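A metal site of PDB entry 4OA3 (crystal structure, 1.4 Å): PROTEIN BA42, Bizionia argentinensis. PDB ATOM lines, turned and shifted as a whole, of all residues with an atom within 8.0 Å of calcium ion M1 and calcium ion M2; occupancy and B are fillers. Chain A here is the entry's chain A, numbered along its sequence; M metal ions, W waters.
Within 4 Å of calcium ion M1: Glu 25, Glu 31, Asp 137, Leu 139 and Asn 141. Along chain A the residues within 4 Å of calcium ion M1 span positions 25 to 141. The nearest printed residue that does not touch calcium ion M1 is Pro 140 (4.2 Å).
Within 4 Å of calcium ion M2: Glu 31, Asp 135, Ile 136 and Asp 137.
The side-chain amide oxygen (OD1) of Asn 141 binds calcium ion M1, 2.3 Å away. OE1 of Glu 31 binds calcium ion M1 (2.4 Å). Calcium ion M1 is bound by O of Leu 139 (2.4 Å). Water W2 is bound to calcium ion M1 (2.4 Å). OD1 of Asp 137 is bound to calcium ion M1 (2.4 Å). Calcium ion M1 is bound by OE1 of Glu 25 (2.5 Å). The side-chain carboxylate (OE2) of Glu 25 is bound to calcium ion M1 (2.5 Å).
OE2 of Glu 25 sits close to N of Ile 32 (3.0 Å). OD2 of Asp 137 is in salt-bridge range of NH1 of Arg 22, at 3.9 Å. The backbone NH of Glu 138 lies close to the side-chain carboxylate of Glu 31. N of Glu 31 lies within hydrogen-bond range of O of Asn 64 (3.2 Å).
Water W2 lies within hydrogen-bond range of the backbone carbonyl oxygen (O) of Ile 32 and the backbone carbonyl oxygen (O) of Pro 140. Water W4 lies within hydrogen-bond range of O of Ser 29 (2.6 Å) and OE1 of Glu 138 (2.8 Å).
Calcium ion M2 is bound by the side-chain carboxylate (OE2) of Glu 31 (2.3 Å), the backbone carbonyl oxygen (O) of Ile 136 (2.4 Å), water W3 (2.4 Å), the side-chain carboxylate (OD2) of Asp 135 (2.4 Å), water W4 (2.4 Å), water W1 (2.5 Å) and the side-chain carboxylate (OD1) of Asp 135 (2.5 Å).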
ATOM      1  N   ILE A  21      19.927   4.993  22.259  1.00  0.00           N
ATOM      2  CA  ILE A  21      20.378   3.631  21.974  1.00  0.00           C
ATOM      3  C   ILE A  21      19.194   2.674  22.085  1.00  0.00           C
ATOM      4  O   ILE A  21      19.016   1.787  21.246  1.00  0.00           O
ATOM      5  CB  ILE A  21      21.543   3.195  22.900  1.00  0.00           C
ATOM      6  CG1 ILE A  21      22.785   4.061  22.561  1.00  0.00           C
ATOM      7  CG2 ILE A  21      21.854   1.708  22.707  1.00  0.00           C
ATOM      8  CD1 ILE A  21      23.977   3.914  23.489  1.00  0.00           C
ATOM      9  N   ARG A  22      18.402   2.814  23.172  1.00  0.00           N
ATOM     10  CA  ARG A  22      17.254   1.915  23.341  1.00  0.00           C
ATOM     11  C   ARG A  22      16.288   2.008  22.172  1.00  0.00           C
ATOM     12  O   ARG A  22      15.833   0.974  21.673  1.00  0.00           O
ATOM     13  CB  ARG A  22      16.530   2.243  24.638  1.00  0.00           C
ATOM     14  CG  ARG A  22      15.434   1.273  24.996  1.00  0.00           C
ATOM     15  CD  ARG A  22      14.998   1.441  26.438  1.00  0.00           C
ATOM     16  NE  ARG A  22      16.115   1.258  27.357  1.00  0.00           N
ATOM     17  CZ  ARG A  22      16.650   0.082  27.713  1.00  0.00           C
ATOM     18  NH1 ARG A  22      16.144  -1.055  27.260  1.00  0.00           N
ATOM     19  NH2 ARG A  22      17.674   0.049  28.550  1.00  0.00           N
ATOM     20  N   ALA A  24      17.048   3.068  19.030  1.00  0.00           N
ATOM     21  CA  ALA A  24      17.708   2.525  17.847  1.00  0.00           C
ATOM     22  C   ALA A  24      17.670   0.999  17.810  1.00  0.00           C
ATOM     23  O   ALA A  24      17.489   0.400  16.758  1.00  0.00           O
ATOM     24  CB  ALA A  24      19.156   3.004  17.811  1.00  0.00           C
ATOM     25  N   GLU A  25      17.843   0.355  18.979  1.00  0.00           N
ATOM     26  CA  GLU A  25      17.830  -1.090  19.059  1.00  0.00           C
ATOM     27  C   GLU A  25      16.426  -1.710  18.954  1.00  0.00           C
ATOM     28  O   GLU A  25      16.312  -2.938  18.979  1.00  0.00           O
ATOM     29  CB  GLU A  25      18.532  -1.546  20.357  1.00  0.00           C
ATOM     30  CG  GLU A  25      20.035  -1.265  20.325  1.00  0.00           C
ATOM     31  CD  GLU A  25      20.811  -1.829  21.492  1.00  0.00           C
ATOM     32  OE1 GLU A  25      20.172  -2.428  22.395  1.00  0.00           O
ATOM     33  OE2 GLU A  25      22.053  -1.672  21.528  1.00  0.00           O
ATOM     34  N   LYS A  26      15.389  -0.903  18.762  1.00  0.00           N
ATOM     35  CA  LYS A  26      14.062  -1.425  18.410  1.00  0.00           C
ATOM     36  C   LYS A  26      13.906  -1.429  16.868  1.00  0.00           C
ATOM     37  O   LYS A  26      12.905  -1.934  16.376  1.00  0.00           O
ATOM     38  CB  LYS A  26      12.958  -0.582  19.024  1.00  0.00           C
ATOM     39  CG  LYS A  26      12.896  -0.630  20.538  1.00  0.00           C
ATOM     40  CD  LYS A  26      11.841   0.346  21.032  1.00  0.00           C
ATOM     41  CE  LYS A  26      11.826   0.474  22.516  1.00  0.00           C
ATOM     42  NZ  LYS A  26      11.223   1.757  22.951  1.00  0.00           N
ATOM     43  N   THR A  28      16.652  -2.372  14.787  1.00  0.00           N
ATOM     44  CA  THR A  28      17.627  -3.330  14.263  1.00  0.00           C
ATOM     45  C   THR A  28      18.013  -4.347  15.321  1.00  0.00           C
ATOM     46  O   THR A  28      17.839  -4.062  16.508  1.00  0.00           O
ATOM     47  CB  THR A  28      18.911  -2.559  13.835  1.00  0.00           C
ATOM     48  OG1 THR A  28      19.874  -3.464  13.295  1.00  0.00           O
ATOM     49  CG2 THR A  28      19.559  -1.780  15.013  1.00  0.00           C
ATOM     50  N   SER A  29      18.538  -5.499  14.900  1.00  0.00           N
ATOM     51  CA  SER A  29      19.126  -6.471  15.810  1.00  0.00           C
ATOM     52  C   SER A  29      20.571  -6.043  16.140  1.00  0.00           C
ATOM     53  O   SER A  29      21.192  -6.641  17.026  1.00  0.00           O
ATOM     54  CB  SER A  29      19.142  -7.874  15.215  1.00  0.00           C
ATOM     55  OG  SER A  29      20.051  -7.957  14.146  1.00  0.00           O
ATOM     56  N   GLY A  30      21.104  -5.012  15.479  1.00  0.00           N
ATOM     57  CA  GLY A  30      22.407  -4.479  15.813  1.00  0.00           C
ATOM     58  C   GLY A  30      22.415  -3.864  17.208  1.00  0.00           C
ATOM     59  O   GLY A  30      21.383  -3.494  17.764  1.00  0.00           O
ATOM     60  N   GLU A  31      23.604  -3.852  17.803  1.00  0.00           N
ATOM     61  CA  GLU A  31      23.790  -3.346  19.156  1.00  0.00           C
ATOM     62  C   GLU A  31      24.750  -2.196  19.149  1.00  0.00           C
ATOM     63  O   GLU A  31      25.784  -2.283  18.478  1.00  0.00           O
ATOM     64  CB  GLU A  31      24.301  -4.453  20.033  1.00  0.00           C
ATOM     65  CG  GLU A  31      23.304  -5.584  20.243  1.00  0.00           C
ATOM     66  CD  GLU A  31      22.341  -5.402  21.399  1.00  0.00           C
ATOM     67  OE1 GLU A  31      22.718  -4.707  22.372  1.00  0.00           O
ATOM     68  OE2 GLU A  31      21.199  -5.941  21.334  1.00  0.00           O
ATOM     69  N   ILE A  32      24.422  -1.111  19.836  1.00  0.00           N
ATOM     70  CA  ILE A  32      25.214   0.110  19.793  1.00  0.00           C
ATOM     71  C   ILE A  32      25.705   0.515  21.154  1.00  0.00           C
ATOM     72  O   ILE A  32      24.948   0.513  22.105  1.00  0.00           O
ATOM     73  CB  ILE A  32      24.369   1.280  19.195  1.00  0.00           C
ATOM     74  CG1 ILE A  32      23.918   0.956  17.771  1.00  0.00           C
ATOM     75  CG2 ILE A  32      25.151   2.607  19.253  1.00  0.00           C
ATOM     76  CD1 ILE A  32      22.750   1.748  17.318  1.00  0.00           C
ATOM     77  N   ARG A  33      27.011   0.893  21.263  1.00  0.00           N
ATOM     78  CA  ARG A  33      27.536   1.536  22.464  1.00  0.00           C
ATOM     79  C   ARG A  33      28.379   2.723  22.110  1.00  0.00           C
ATOM     80  O   ARG A  33      28.923   2.821  20.997  1.00  0.00           O
ATOM     81  CB  ARG A  33      28.395   0.609  23.336  1.00  0.00           C
ATOM     82  CG  ARG A  33      27.604  -0.579  23.865  1.00  0.00           C
ATOM     83  CD  ARG A  33      28.308  -1.332  24.967  1.00  0.00           C
ATOM     84  NE  ARG A  33      28.407  -0.486  26.162  1.00  0.00           N
ATOM     85  CZ  ARG A  33      29.147  -0.769  27.212  1.00  0.00           C
ATOM     86  NH1 ARG A  33      29.876  -1.874  27.242  1.00  0.00           N
ATOM     87  NH2 ARG A  33      29.189   0.064  28.242  1.00  0.00           N
ATOM     88  N   THR A  60      27.712 -10.782  20.340  1.00  0.00           N
ATOM     89  CA  THR A  60      26.408 -10.675  19.700  1.00  0.00           C
ATOM     90  C   THR A  60      26.306 -11.897  18.781  1.00  0.00           C
ATOM     91  O   THR A  60      27.309 -12.314  18.194  1.00  0.00           O
ATOM     92  CB  THR A  60      26.235  -9.356  18.933  1.00  0.00           C
ATOM     93  OG1 THR A  60      27.087  -9.319  17.781  1.00  0.00           O
ATOM     94  CG2 THR A  60      26.409  -8.135  19.817  1.00  0.00           C
ATOM     95  N   ASN A  64      27.213  -8.074  15.085  1.00  0.00           N
ATOM     96  CA  ASN A  64      26.713  -6.811  14.622  1.00  0.00           C
ATOM     97  C   ASN A  64      26.666  -5.695  15.675  1.00  0.00           C
ATOM     98  O   ASN A  64      25.800  -4.843  15.641  1.00  0.00           O
ATOM     99  CB  ASN A  64      25.381  -6.986  13.906  1.00  0.00           C
ATOM    100  CG  ASN A  64      24.298  -7.535  14.787  1.00  0.00           C
ATOM    101  OD1 ASN A  64      24.524  -7.940  15.901  1.00  0.00           O
ATOM    102  ND2 ASN A  64      23.067  -7.501  14.295  1.00  0.00           N
ATOM    103  N   TRP A 131      15.189  -5.907  13.027  1.00  0.00           N
ATOM    104  CA  TRP A 131      14.767  -6.252  14.376  1.00  0.00           C
ATOM    105  C   TRP A 131      13.789  -7.441  14.296  1.00  0.00           C
ATOM    106  O   TRP A 131      12.982  -7.516  13.366  1.00  0.00           O
ATOM    107  CB  TRP A 131      14.082  -5.055  15.029  1.00  0.00           C
ATOM    108  CG  TRP A 131      13.617  -5.288  16.425  1.00  0.00           C
ATOM    109  CD1 TRP A 131      14.311  -5.086  17.573  1.00  0.00           C
ATOM    110  CD2 TRP A 131      12.300  -5.722  16.816  1.00  0.00           C
ATOM    111  NE1 TRP A 131      13.534  -5.421  18.665  1.00  0.00           N
ATOM    112  CE2 TRP A 131      12.299  -5.829  18.220  1.00  0.00           C
ATOM    113  CE3 TRP A 131      11.132  -6.046  16.110  1.00  0.00           C
ATOM    114  CZ2 TRP A 131      11.166  -6.208  18.937  1.00  0.00           C
ATOM    115  CZ3 TRP A 131      10.023  -6.472  16.824  1.00  0.00           C
ATOM    116  CH2 TRP A 131      10.027  -6.489  18.221  1.00  0.00           C
ATOM    117  N   LYS A 132      13.921  -8.372  15.239  1.00  0.00           N
ATOM    118  CA  LYS A 132      13.089  -9.571  15.332  1.00  0.00           C
ATOM    119  C   LYS A 132      12.358  -9.546  16.658  1.00  0.00           C
ATOM    120  O   LYS A 132      12.883  -9.031  17.650  1.00  0.00           O
ATOM    121  CB  LYS A 132      13.938 -10.839  15.265  1.00  0.00           C
ATOM    122  CG  LYS A 132      14.846 -10.940  14.043  1.00  0.00           C
ATOM    123  CD  LYS A 132      14.085 -10.994  12.742  1.00  0.00           C
ATOM    124  CE  LYS A 132      14.984 -11.309  11.572  1.00  0.00           C
ATOM    125  NZ  LYS A 132      15.589 -12.670  11.656  1.00  0.00           N
ATOM    126  N   ASP A 134      11.814 -11.630  19.127  1.00  0.00           N
ATOM    127  CA  ASP A 134      12.498 -12.212  20.280  1.00  0.00           C
ATOM    128  C   ASP A 134      13.914 -11.594  20.441  1.00  0.00           C
ATOM    129  O   ASP A 134      14.828 -12.239  20.967  1.00  0.00           O
ATOM    130  CB  ASP A 134      12.554 -13.755  20.147  1.00  0.00           C
ATOM    131  CG  ASP A 134      13.038 -14.276  18.803  1.00  0.00           C
ATOM    132  OD1 ASP A 134      13.120 -13.465  17.854  1.00  0.00           O
ATOM    133  OD2 ASP A 134      13.285 -15.495  18.687  1.00  0.00           O
ATOM    134  N   ASP A 135      14.079 -10.323  20.015  1.00  0.00           N
ATOM    135  CA  ASP A 135      15.356  -9.632  20.148  1.00  0.00           C
ATOM    136  C   ASP A 135      15.844  -9.709  21.574  1.00  0.00           C
ATOM    137  O   ASP A 135      15.058  -9.535  22.506  1.00  0.00           O
ATOM    138  CB  ASP A 135      15.206  -8.137  19.797  1.00  0.00           C
ATOM    139  CG  ASP A 135      16.526  -7.380  19.963  1.00  0.00           C
ATOM    140  OD1 ASP A 135      17.346  -7.432  19.034  1.00  0.00           O
ATOM    141  OD2 ASP A 135      16.705  -6.736  21.013  1.00  0.00           O
ATOM    142  N   ILE A 136      17.137  -9.913  21.729  1.00  0.00           N
ATOM    143  CA  ILE A 136      17.821  -9.926  23.020  1.00  0.00           C
ATOM    144  C   ILE A 136      18.615  -8.598  23.096  1.00  0.00           C
ATOM    145  O   ILE A 136      19.208  -8.202  22.092  1.00  0.00           O
ATOM    146  CB  ILE A 136      18.779 -11.131  23.070  1.00  0.00           C
ATOM    147  CG1 ILE A 136      17.971 -12.473  23.008  1.00  0.00           C
ATOM    148  CG2 ILE A 136      19.691 -11.071  24.328  1.00  0.00           C
ATOM    149  CD1 ILE A 136      18.819 -13.664  22.942  1.00  0.00           C
ATOM    150  N   ASP A 137      18.657  -7.949  24.266  1.00  0.00           N
ATOM    151  CA  ASP A 137      19.488  -6.745  24.450  1.00  0.00           C
ATOM    152  C   ASP A 137      20.864  -7.331  24.847  1.00  0.00           C
ATOM    153  O   ASP A 137      21.113  -7.657  26.000  1.00  0.00           O
ATOM    154  CB  ASP A 137      18.903  -5.822  25.508  1.00  0.00           C
ATOM    155  CG  ASP A 137      19.519  -4.446  25.531  1.00  0.00           C
ATOM    156  OD1 ASP A 137      20.631  -4.270  24.958  1.00  0.00           O
ATOM    157  OD2 ASP A 137      18.911  -3.539  26.126  1.00  0.00           O
ATOM    158  N   GLU A 138      21.670  -7.619  23.830  1.00  0.00           N
ATOM    159  CA  GLU A 138      22.927  -8.358  23.978  1.00  0.00           C
ATOM    160  C   GLU A 138      24.059  -7.621  24.648  1.00  0.00           C
ATOM    161  O   GLU A 138      24.843  -8.244  25.362  1.00  0.00           O
ATOM    162  CB  GLU A 138      23.371  -8.882  22.607  1.00  0.00           C
ATOM    163  CG  GLU A 138      22.400  -9.892  21.991  1.00  0.00           C
ATOM    164  CD  GLU A 138      22.743 -10.292  20.580  1.00  0.00           C
ATOM    165  OE1 GLU A 138      22.668  -9.425  19.685  1.00  0.00           O
ATOM    166  OE2 GLU A 138      23.035 -11.499  20.350  1.00  0.00           O
ATOM    167  N   LEU A 139      24.140  -6.311  24.427  1.00  0.00           N
ATOM    168  CA  LEU A 139      25.186  -5.488  25.003  1.00  0.00           C
ATOM    169  C   LEU A 139      24.549  -4.404  25.839  1.00  0.00           C
ATOM    170  O   LEU A 139      23.526  -3.854  25.452  1.00  0.00           O
ATOM    171  CB  LEU A 139      26.032  -4.813  23.925  1.00  0.00           C
ATOM    172  CG  LEU A 139      26.683  -5.750  22.895  1.00  0.00           C
ATOM    173  CD1 LEU A 139      27.476  -4.947  21.852  1.00  0.00           C
ATOM    174  CD2 LEU A 139      27.579  -6.786  23.542  1.00  0.00           C
ATOM    175  N   PRO A 140      25.153  -4.018  26.985  1.00  0.00           N
ATOM    176  CA  PRO A 140      24.603  -2.905  27.753  1.00  0.00           C
ATOM    177  C   PRO A 140      24.579  -1.592  26.978  1.00  0.00           C
ATOM    178  O   PRO A 140      25.380  -1.390  26.049  1.00  0.00           O
ATOM    179  CB  PRO A 140      25.510  -2.824  28.987  1.00  0.00           C
ATOM    180  CG  PRO A 140      26.667  -3.538  28.666  1.00  0.00           C
ATOM    181  CD  PRO A 140      26.394  -4.524  27.564  1.00  0.00           C
ATOM    182  N   ASN A 141      23.614  -0.738  27.310  1.00  0.00           N
ATOM    183  CA  ASN A 141      23.454   0.540  26.618  1.00  0.00           C
ATOM    184  C   ASN A 141      24.206   1.654  27.341  1.00  0.00           C
ATOM    185  O   ASN A 141      24.263   2.751  26.830  1.00  0.00           O
ATOM    186  CB  ASN A 141      21.998   0.883  26.473  1.00  0.00           C
ATOM    187  CG  ASN A 141      21.195  -0.115  25.674  1.00  0.00           C
ATOM    188  OD1 ASN A 141      21.711  -0.985  24.976  1.00  0.00           O
ATOM    189  ND2 ASN A 141      19.875   0.102  25.701  1.00  0.00           N
ATOM    190  N   THR A 142      24.835   1.319  28.475  1.00  0.00           N
ATOM    191  CA  THR A 142      25.655   2.229  29.296  1.00  0.00           C
ATOM    192  C   THR A 142      26.711   2.890  28.452  1.00  0.00           C
ATOM    193  O   THR A 142      27.387   2.200  27.677  1.00  0.00           O
ATOM    194  CB  THR A 142      26.448   1.375  30.328  1.00  0.00           C
ATOM    195  OG1 THR A 142      25.651   0.353  30.855  1.00  0.00           O
ATOM    196  CG2 THR A 142      27.039   2.167  31.472  1.00  0.00           C
HETATM  197 CA    CA M   1      22.162  -2.866  23.757  1.00  0.00          CA
HETATM  198 CA    CA M   2      19.069  -6.428  20.509  1.00  0.00          CA
HETATM  199  O   HOH W   1      18.472  -4.662  22.143  1.00  0.00           O
HETATM  200  O   HOH W   2      24.273  -1.775  23.486  1.00  0.00           O
HETATM  201  O   HOH W   3      19.203  -4.687  18.887  1.00  0.00           O
HETATM  202  O   HOH W   4      20.368  -7.963  19.110  1.00  0.00           O
